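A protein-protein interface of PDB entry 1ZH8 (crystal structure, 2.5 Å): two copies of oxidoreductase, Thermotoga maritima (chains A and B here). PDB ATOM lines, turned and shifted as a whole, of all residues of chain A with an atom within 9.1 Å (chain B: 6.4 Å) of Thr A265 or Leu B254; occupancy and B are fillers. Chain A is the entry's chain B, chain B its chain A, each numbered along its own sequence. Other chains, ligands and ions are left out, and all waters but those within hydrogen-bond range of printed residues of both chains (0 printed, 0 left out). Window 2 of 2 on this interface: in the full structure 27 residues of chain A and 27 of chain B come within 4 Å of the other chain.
Among the printed residues, merely in contact across the chains: Val A164 with Leu B224 (3.6 Å), Phe A165 with Trp B171 (3.7 Å), Thr A263 with Trp B171 (3.9 Å), Phe A165 with Phe B233 (3.9 Å), Gly A264 with Leu B254 (3.9 Å), Val A164 with Leu B254 (3.97 Å) and Thr A265 with Leu B254 (3.999 Å).
Asp A162 touches none of the printed residues of chain B.
Of the printed residues of chain B, Thr A263 touches Trp B171 (3.9 Å).
Printed residues of chain B within 4 Å of Thr A265: Leu B254.
Printed residues of chain A within 4 Å of Trp B171: Phe A165 and Thr A263.
Of the printed residues of chain A, Leu B224 touches Val A164 (3.6 Å).
Of the printed residues of chain A, Phe B233 touches Phe A165 (3.9 Å).
Printed residues of chain A within 4 Å of Leu B254: Val A164, Gly A264 and Thr A265.
Gly B256 touches none of the printed residues of chain A.
The nearest printed residue of chain A that does not touch Leu B254 is Thr A263 (4.9 Å).
Along chain B the printed residues that touch a printed residue of chain A span positions 171 to 254.
Of the 16 printed residues of chain A, 5 touch a printed residue of chain B.
Printed residues of chain A that touch a printed residue of chain B: Val A164, Phe A165, Thr A263, Gly A264 and Thr A265.
Among the printed residues, no Asp or Glu carboxylate lies within 4 Å of a Lys or Arg side-chain nitrogen of the other chain.
O of Leu B254 lies within hydrogen-bond range of N of Gly B173.
The side-chain hydroxyl (OG) of Ser B251 is in hydrogen-bond range of the backbone NH (N) of Leu B254 (3.0 Å).
O of Ile A160 is in hydrogen-bond range of N of Thr A265 (3.2 Å).
The backbone carbonyl oxygen (O) of Asp A162 lies within hydrogen-bond range of the backbone NH (N) of Thr A265 (3.0 Å).
The backbone NH (N) of Val A164 is in hydrogen-bond range of the backbone carbonyl oxygen (O) of Thr A263, at 2.8 Å.
The backbone carbonyl oxygen (O) of Phe A165 is in hydrogen-bond range of the backbone NH (N) of Thr A263 (2.8 Å).
No position is printed for both chains.
Of the 7 pairs that touch across the chains among the printed residues, none has its exchanged pair printed and touching as well.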
ATOM      1  N   GLY A 158     -29.067 -27.866  -3.151  1.00  0.00           N
ATOM      2  CA  GLY A 158     -28.154 -27.558  -4.251  1.00  0.00           C
ATOM      3  C   GLY A 158     -28.501 -26.345  -5.103  1.00  0.00           C
ATOM      4  O   GLY A 158     -27.974 -26.202  -6.214  1.00  0.00           O
ATOM      5  N   ALA A 159     -29.347 -25.450  -4.585  1.00  0.00           N
ATOM      6  CA  ALA A 159     -29.786 -24.263  -5.343  1.00  0.00           C
ATOM      7  C   ALA A 159     -28.653 -23.313  -5.763  1.00  0.00           C
ATOM      8  O   ALA A 159     -28.762 -22.651  -6.793  1.00  0.00           O
ATOM      9  CB  ALA A 159     -30.884 -23.501  -4.600  1.00  0.00           C
ATOM     10  N   ILE A 160     -27.579 -23.242  -4.981  1.00  0.00           N
ATOM     11  CA  ILE A 160     -26.423 -22.422  -5.377  1.00  0.00           C
ATOM     12  C   ILE A 160     -25.160 -23.246  -5.721  1.00  0.00           C
ATOM     13  O   ILE A 160     -24.057 -22.697  -5.807  1.00  0.00           O
ATOM     14  CB  ILE A 160     -26.089 -21.348  -4.321  1.00  0.00           C
ATOM     15  CG1 ILE A 160     -25.790 -21.999  -2.976  1.00  0.00           C
ATOM     16  CG2 ILE A 160     -27.228 -20.362  -4.193  1.00  0.00           C
ATOM     17  CD1 ILE A 160     -25.132 -21.057  -1.947  1.00  0.00           C
ATOM     18  N   GLY A 161     -25.329 -24.552  -5.927  1.00  0.00           N
ATOM     19  CA  GLY A 161     -24.195 -25.451  -6.176  1.00  0.00           C
ATOM     20  C   GLY A 161     -23.443 -25.739  -4.892  1.00  0.00           C
ATOM     21  O   GLY A 161     -24.035 -25.741  -3.815  1.00  0.00           O
ATOM     22  N   ASP A 162     -22.135 -25.973  -4.994  1.00  0.00           N
ATOM     23  CA  ASP A 162     -21.306 -26.180  -3.794  1.00  0.00           C
ATOM     24  C   ASP A 162     -21.038 -24.844  -3.107  1.00  0.00           C
ATOM     25  O   ASP A 162     -20.541 -23.919  -3.750  1.00  0.00           O
ATOM     26  CB  ASP A 162     -19.985 -26.876  -4.149  1.00  0.00           C
ATOM     27  CG  ASP A 162     -20.197 -28.200  -4.862  1.00  0.00           C
ATOM     28  OD1 ASP A 162     -21.071 -28.992  -4.431  1.00  0.00           O
ATOM     29  OD2 ASP A 162     -19.491 -28.451  -5.860  1.00  0.00           O
ATOM     30  N   PRO A 163     -21.404 -24.720  -1.816  1.00  0.00           N
ATOM     31  CA  PRO A 163     -21.188 -23.479  -1.051  1.00  0.00           C
ATOM     32  C   PRO A 163     -19.712 -23.117  -0.922  1.00  0.00           C
ATOM     33  O   PRO A 163     -18.897 -23.954  -0.535  1.00  0.00           O
ATOM     34  CB  PRO A 163     -21.789 -23.801   0.321  1.00  0.00           C
ATOM     35  CG  PRO A 163     -22.739 -24.917   0.044  1.00  0.00           C
ATOM     36  CD  PRO A 163     -22.100 -25.733  -1.012  1.00  0.00           C
ATOM     37  N   VAL A 164     -19.375 -21.877  -1.255  1.00  0.00           N
ATOM     38  CA  VAL A 164     -17.973 -21.469  -1.289  1.00  0.00           C
ATOM     39  C   VAL A 164     -17.636 -20.499  -0.165  1.00  0.00           C
ATOM     40  O   VAL A 164     -16.609 -20.670   0.517  1.00  0.00           O
ATOM     41  CB  VAL A 164     -17.599 -20.847  -2.650  1.00  0.00           C
ATOM     42  CG1 VAL A 164     -16.174 -20.312  -2.623  1.00  0.00           C
ATOM     43  CG2 VAL A 164     -17.796 -21.868  -3.774  1.00  0.00           C
ATOM     44  N   PHE A 165     -18.513 -19.507   0.027  1.00  0.00           N
ATOM     45  CA  PHE A 165     -18.257 -18.370   0.919  1.00  0.00           C
ATOM     46  C   PHE A 165     -19.533 -17.756   1.499  1.00  0.00           C
ATOM     47  O   PHE A 165     -20.442 -17.333   0.761  1.00  0.00           O
ATOM     48  CB  PHE A 165     -17.463 -17.297   0.163  1.00  0.00           C
ATOM     49  CG  PHE A 165     -17.142 -16.069   0.974  1.00  0.00           C
ATOM     50  CD1 PHE A 165     -16.128 -16.096   1.926  1.00  0.00           C
ATOM     51  CD2 PHE A 165     -17.839 -14.869   0.761  1.00  0.00           C
ATOM     52  CE1 PHE A 165     -15.804 -14.929   2.697  1.00  0.00           C
ATOM     53  CE2 PHE A 165     -17.545 -13.705   1.525  1.00  0.00           C
ATOM     54  CZ  PHE A 165     -16.508 -13.743   2.504  1.00  0.00           C
ATOM     55  N   ILE A 262     -24.548 -15.917   1.012  1.00  0.00           N
ATOM     56  CA  ILE A 262     -23.845 -17.173   0.801  1.00  0.00           C
ATOM     57  C   ILE A 262     -23.674 -17.340  -0.704  1.00  0.00           C
ATOM     58  O   ILE A 262     -24.646 -17.357  -1.446  1.00  0.00           O
ATOM     59  CB  ILE A 262     -24.598 -18.390   1.415  1.00  0.00           C
ATOM     60  CG1 ILE A 262     -24.961 -18.113   2.861  1.00  0.00           C
ATOM     61  CG2 ILE A 262     -23.748 -19.650   1.324  1.00  0.00           C
ATOM     62  CD1 ILE A 262     -25.803 -19.174   3.488  1.00  0.00           C
ATOM     63  N   THR A 263     -22.431 -17.437  -1.142  1.00  0.00           N
ATOM     64  CA  THR A 263     -22.113 -17.632  -2.553  1.00  0.00           C
ATOM     65  C   THR A 263     -21.646 -19.054  -2.789  1.00  0.00           C
ATOM     66  O   THR A 263     -20.853 -19.612  -2.006  1.00  0.00           O
ATOM     67  CB  THR A 263     -21.014 -16.668  -3.024  1.00  0.00           C
ATOM     68  OG1 THR A 263     -21.304 -15.357  -2.531  1.00  0.00           O
ATOM     69  CG2 THR A 263     -20.927 -16.617  -4.551  1.00  0.00           C
ATOM     70  N   GLY A 264     -22.142 -19.638  -3.875  1.00  0.00           N
ATOM     71  CA  GLY A 264     -21.717 -20.964  -4.284  1.00  0.00           C
ATOM     72  C   GLY A 264     -21.098 -20.975  -5.657  1.00  0.00           C
ATOM     73  O   GLY A 264     -20.840 -19.916  -6.238  1.00  0.00           O
ATOM     74  N   THR A 265     -20.877 -22.182  -6.175  1.00  0.00           N
ATOM     75  CA  THR A 265     -20.307 -22.383  -7.508  1.00  0.00           C
ATOM     76  C   THR A 265     -21.331 -22.054  -8.593  1.00  0.00           C
ATOM     77  O   THR A 265     -20.971 -21.662  -9.702  1.00  0.00           O
ATOM     78  CB  THR A 265     -19.801 -23.848  -7.705  1.00  0.00           C
ATOM     79  OG1 THR A 265     -20.868 -24.775  -7.456  1.00  0.00           O
ATOM     80  CG2 THR A 265     -18.608 -24.167  -6.763  1.00  0.00           C
ATOM     81  N   LYS A 266     -22.608 -22.200  -8.254  1.00  0.00           N
ATOM     82  CA  LYS A 266     -23.686 -22.049  -9.231  1.00  0.00           C
ATOM     83  C   LYS A 266     -24.541 -20.795  -9.018  1.00  0.00           C
ATOM     84  O   LYS A 266     -25.296 -20.419  -9.904  1.00  0.00           O
ATOM     85  CB  LYS A 266     -24.579 -23.305  -9.267  1.00  0.00           C
ATOM     86  CG  LYS A 266     -23.924 -24.550  -9.884  1.00  0.00           C
ATOM     87  CD  LYS A 266     -24.968 -25.586 -10.347  1.00  0.00           C
ATOM     88  N   GLY A 267     -24.412 -20.139  -7.863  1.00  0.00           N
ATOM     89  CA  GLY A 267     -25.280 -19.001  -7.551  1.00  0.00           C
ATOM     90  C   GLY A 267     -25.039 -18.246  -6.257  1.00  0.00           C
ATOM     91  O   GLY A 267     -23.990 -18.378  -5.638  1.00  0.00           O
ATOM     92  N   LYS A 268     -26.034 -17.456  -5.849  1.00  0.00           N
ATOM     93  CA  LYS A 268     -25.898 -16.500  -4.740  1.00  0.00           C
ATOM     94  C   LYS A 268     -27.237 -16.300  -4.001  1.00  0.00           C
ATOM     95  O   LYS A 268     -28.241 -15.963  -4.628  1.00  0.00           O
ATOM     96  CB  LYS A 268     -25.374 -15.155  -5.298  1.00  0.00           C
ATOM     97  CG  LYS A 268     -25.347 -13.981  -4.312  1.00  0.00           C
ATOM     98  N   ASN A 279     -30.124 -15.413  -6.406  1.00  0.00           N
ATOM     99  CA  ASN A 279     -29.656 -14.699  -7.594  1.00  0.00           C
ATOM    100  C   ASN A 279     -30.458 -13.409  -7.803  1.00  0.00           C
ATOM    101  O   ASN A 279     -30.322 -12.483  -7.009  1.00  0.00           O
ATOM    102  CB  ASN A 279     -29.640 -15.623  -8.821  1.00  0.00           C
ATOM    103  CG  ASN A 279     -28.866 -16.910  -8.558  1.00  0.00           C
ATOM    104  OD1 ASN A 279     -27.734 -16.886  -8.041  1.00  0.00           O
ATOM    105  ND2 ASN A 279     -29.479 -18.038  -8.873  1.00  0.00           N
ATOM    106  N   ILE B 170     -14.114  -8.823  -3.713  1.00  0.00           N
ATOM    107  CA  ILE B 170     -13.960  -8.689  -5.148  1.00  0.00           C
ATOM    108  C   ILE B 170     -14.346  -9.996  -5.825  1.00  0.00           C
ATOM    109  O   ILE B 170     -13.859 -11.057  -5.455  1.00  0.00           O
ATOM    110  CB  ILE B 170     -12.510  -8.294  -5.499  1.00  0.00           C
ATOM    111  CG1 ILE B 170     -12.117  -7.029  -4.731  1.00  0.00           C
ATOM    112  CG2 ILE B 170     -12.318  -8.139  -7.028  1.00  0.00           C
ATOM    113  CD1 ILE B 170     -10.654  -6.761  -4.744  1.00  0.00           C
ATOM    114  N   TRP B 171     -15.221  -9.923  -6.819  1.00  0.00           N
ATOM    115  CA  TRP B 171     -15.616 -11.130  -7.526  1.00  0.00           C
ATOM    116  C   TRP B 171     -15.380 -10.948  -9.011  1.00  0.00           C
ATOM    117  O   TRP B 171     -16.222 -10.407  -9.705  1.00  0.00           O
ATOM    118  CB  TRP B 171     -17.074 -11.465  -7.232  1.00  0.00           C
ATOM    119  CG  TRP B 171     -17.378 -11.670  -5.772  1.00  0.00           C
ATOM    120  CD1 TRP B 171     -17.756 -10.715  -4.856  1.00  0.00           C
ATOM    121  CD2 TRP B 171     -17.354 -12.912  -5.061  1.00  0.00           C
ATOM    122  NE1 TRP B 171     -17.958 -11.291  -3.625  1.00  0.00           N
ATOM    123  CE2 TRP B 171     -17.718 -12.636  -3.724  1.00  0.00           C
ATOM    124  CE3 TRP B 171     -17.058 -14.231  -5.425  1.00  0.00           C
ATOM    125  CZ2 TRP B 171     -17.793 -13.634  -2.753  1.00  0.00           C
ATOM    126  CZ3 TRP B 171     -17.131 -15.224  -4.459  1.00  0.00           C
ATOM    127  CH2 TRP B 171     -17.494 -14.920  -3.138  1.00  0.00           C
ATOM    128  N   VAL B 172     -14.225 -11.393  -9.497  1.00  0.00           N
ATOM    129  CA  VAL B 172     -13.813 -11.105 -10.883  1.00  0.00           C
ATOM    130  C   VAL B 172     -14.590 -11.873 -11.970  1.00  0.00           C
ATOM    131  O   VAL B 172     -14.776 -11.358 -13.076  1.00  0.00           O
ATOM    132  CB  VAL B 172     -12.277 -11.218 -11.062  1.00  0.00           C
ATOM    133  CG1 VAL B 172     -11.829 -10.506 -12.330  1.00  0.00           C
ATOM    134  CG2 VAL B 172     -11.548 -10.610  -9.853  1.00  0.00           C
ATOM    135  N   GLY B 173     -15.063 -13.080 -11.655  1.00  0.00           N
ATOM    136  CA  GLY B 173     -15.789 -13.918 -12.612  1.00  0.00           C
ATOM    137  C   GLY B 173     -15.091 -14.166 -13.950  1.00  0.00           C
ATOM    138  O   GLY B 173     -15.741 -14.164 -15.010  1.00  0.00           O
ATOM    139  N   MET B 174     -13.775 -14.392 -13.917  1.00  0.00           N
ATOM    140  CA  MET B 174     -13.038 -14.680 -15.148  1.00  0.00           C
ATOM    141  C   MET B 174     -13.502 -16.013 -15.691  1.00  0.00           C
ATOM    142  O   MET B 174     -13.681 -16.965 -14.933  1.00  0.00           O
ATOM    143  CB  MET B 174     -11.535 -14.747 -14.910  1.00  0.00           C
ATOM    144  CG  MET B 174     -10.898 -13.458 -14.492  1.00  0.00           C
ATOM    145  SD  MET B 174      -8.986 -13.742 -14.142  1.00  0.00           S
ATOM    146  CE  MET B 174      -8.298 -11.967 -14.586  1.00  0.00           C
ATOM    147  N   LEU B 224     -10.117 -23.096  -6.820  1.00  0.00           N
ATOM    148  CA  LEU B 224     -11.519 -23.479  -7.100  1.00  0.00           C
ATOM    149  C   LEU B 224     -11.851 -23.675  -8.586  1.00  0.00           C
ATOM    150  O   LEU B 224     -12.859 -24.292  -8.935  1.00  0.00           O
ATOM    151  CB  LEU B 224     -12.478 -22.425  -6.535  1.00  0.00           C
ATOM    152  CG  LEU B 224     -12.527 -22.107  -5.044  1.00  0.00           C
ATOM    153  CD1 LEU B 224     -13.391 -20.880  -4.877  1.00  0.00           C
ATOM    154  CD2 LEU B 224     -13.082 -23.313  -4.250  1.00  0.00           C
ATOM    155  N   PHE B 233      -8.880 -18.208  -5.066  1.00  0.00           N
ATOM    156  CA  PHE B 233      -9.766 -17.712  -4.035  1.00  0.00           C
ATOM    157  C   PHE B 233      -8.978 -17.403  -2.772  1.00  0.00           C
ATOM    158  O   PHE B 233      -8.094 -18.151  -2.380  1.00  0.00           O
ATOM    159  CB  PHE B 233     -10.885 -18.706  -3.746  1.00  0.00           C
ATOM    160  CG  PHE B 233     -11.791 -18.280  -2.623  1.00  0.00           C
ATOM    161  CD1 PHE B 233     -11.489 -18.609  -1.300  1.00  0.00           C
ATOM    162  CD2 PHE B 233     -12.922 -17.533  -2.876  1.00  0.00           C
ATOM    163  CE1 PHE B 233     -12.304 -18.213  -0.263  1.00  0.00           C
ATOM    164  CE2 PHE B 233     -13.750 -17.126  -1.832  1.00  0.00           C
ATOM    165  CZ  PHE B 233     -13.439 -17.468  -0.525  1.00  0.00           C
ATOM    166  N   SER B 251     -12.459 -13.809  -5.270  1.00  0.00           N
ATOM    167  CA  SER B 251     -12.514 -14.985  -6.130  1.00  0.00           C
ATOM    168  C   SER B 251     -12.233 -14.516  -7.528  1.00  0.00           C
ATOM    169  O   SER B 251     -12.908 -13.643  -8.035  1.00  0.00           O
ATOM    170  CB  SER B 251     -13.889 -15.625  -6.101  1.00  0.00           C
ATOM    171  OG  SER B 251     -13.943 -16.707  -7.019  1.00  0.00           O
ATOM    172  N   TYR B 252     -11.222 -15.075  -8.164  1.00  0.00           N
ATOM    173  CA  TYR B 252     -10.985 -14.707  -9.541  1.00  0.00           C
ATOM    174  C   TYR B 252     -11.966 -15.387 -10.496  1.00  0.00           C
ATOM    175  O   TYR B 252     -12.130 -14.923 -11.625  1.00  0.00           O
ATOM    176  CB  TYR B 252      -9.549 -14.971  -9.909  1.00  0.00           C
ATOM    177  CG  TYR B 252      -8.642 -13.938  -9.311  1.00  0.00           C
ATOM    178  CD1 TYR B 252      -8.198 -14.057  -7.998  1.00  0.00           C
ATOM    179  CD2 TYR B 252      -8.215 -12.840 -10.059  1.00  0.00           C
ATOM    180  CE1 TYR B 252      -7.353 -13.095  -7.432  1.00  0.00           C
ATOM    181  CE2 TYR B 252      -7.389 -11.876  -9.512  1.00  0.00           C
ATOM    182  CZ  TYR B 252      -6.960 -12.008  -8.197  1.00  0.00           C
ATOM    183  OH  TYR B 252      -6.126 -11.064  -7.647  1.00  0.00           O
ATOM    184  N   SER B 253     -12.655 -16.438 -10.047  1.00  0.00           N
ATOM    185  CA  SER B 253     -13.480 -17.239 -10.967  1.00  0.00           C
ATOM    186  C   SER B 253     -14.993 -17.056 -10.799  1.00  0.00           C
ATOM    187  O   SER B 253     -15.736 -17.221 -11.752  1.00  0.00           O
ATOM    188  CB  SER B 253     -13.079 -18.715 -10.870  1.00  0.00           C
ATOM    189  OG  SER B 253     -14.201 -19.570 -10.792  1.00  0.00           O
ATOM    190  N   LEU B 254     -15.443 -16.679  -9.606  1.00  0.00           N
ATOM    191  CA  LEU B 254     -16.874 -16.503  -9.352  1.00  0.00           C
ATOM    192  C   LEU B 254     -17.362 -15.054  -9.479  1.00  0.00           C
ATOM    193  O   LEU B 254     -16.577 -14.116  -9.335  1.00  0.00           O
ATOM    194  CB  LEU B 254     -17.232 -17.082  -7.980  1.00  0.00           C
ATOM    195  CG  LEU B 254     -16.898 -18.569  -7.806  1.00  0.00           C
ATOM    196  CD1 LEU B 254     -16.978 -18.959  -6.348  1.00  0.00           C
ATOM    197  CD2 LEU B 254     -17.800 -19.458  -8.662  1.00  0.00           C
ATOM    198  N   LYS B 255     -18.663 -14.906  -9.745  1.00  0.00           N
ATOM    199  CA  LYS B 255     -19.337 -13.627 -10.002  1.00  0.00           C
ATOM    200  C   LYS B 255     -19.999 -13.032  -8.765  1.00  0.00           C
ATOM    201  O   LYS B 255     -20.477 -13.750  -7.874  1.00  0.00           O
ATOM    202  CB  LYS B 255     -20.425 -13.809 -11.063  1.00  0.00           C
ATOM    203  CG  LYS B 255     -19.966 -13.666 -12.507  1.00  0.00           C
ATOM    204  CD  LYS B 255     -21.138 -13.897 -13.487  1.00  0.00           C
ATOM    205  CE  LYS B 255     -20.676 -13.793 -14.949  1.00  0.00           C
ATOM    206  NZ  LYS B 255     -21.819 -13.568 -15.893  1.00  0.00           N
ATOM    207  N   GLY B 256     -20.052 -11.705  -8.739  1.00  0.00           N
ATOM    208  CA  GLY B 256     -20.748 -10.968  -7.681  1.00  0.00           C
ATOM    209  C   GLY B 256     -20.435  -9.484  -7.760  1.00  0.00           C
ATOM    210  O   GLY B 256     -19.745  -9.018  -8.692  1.00  0.00           O
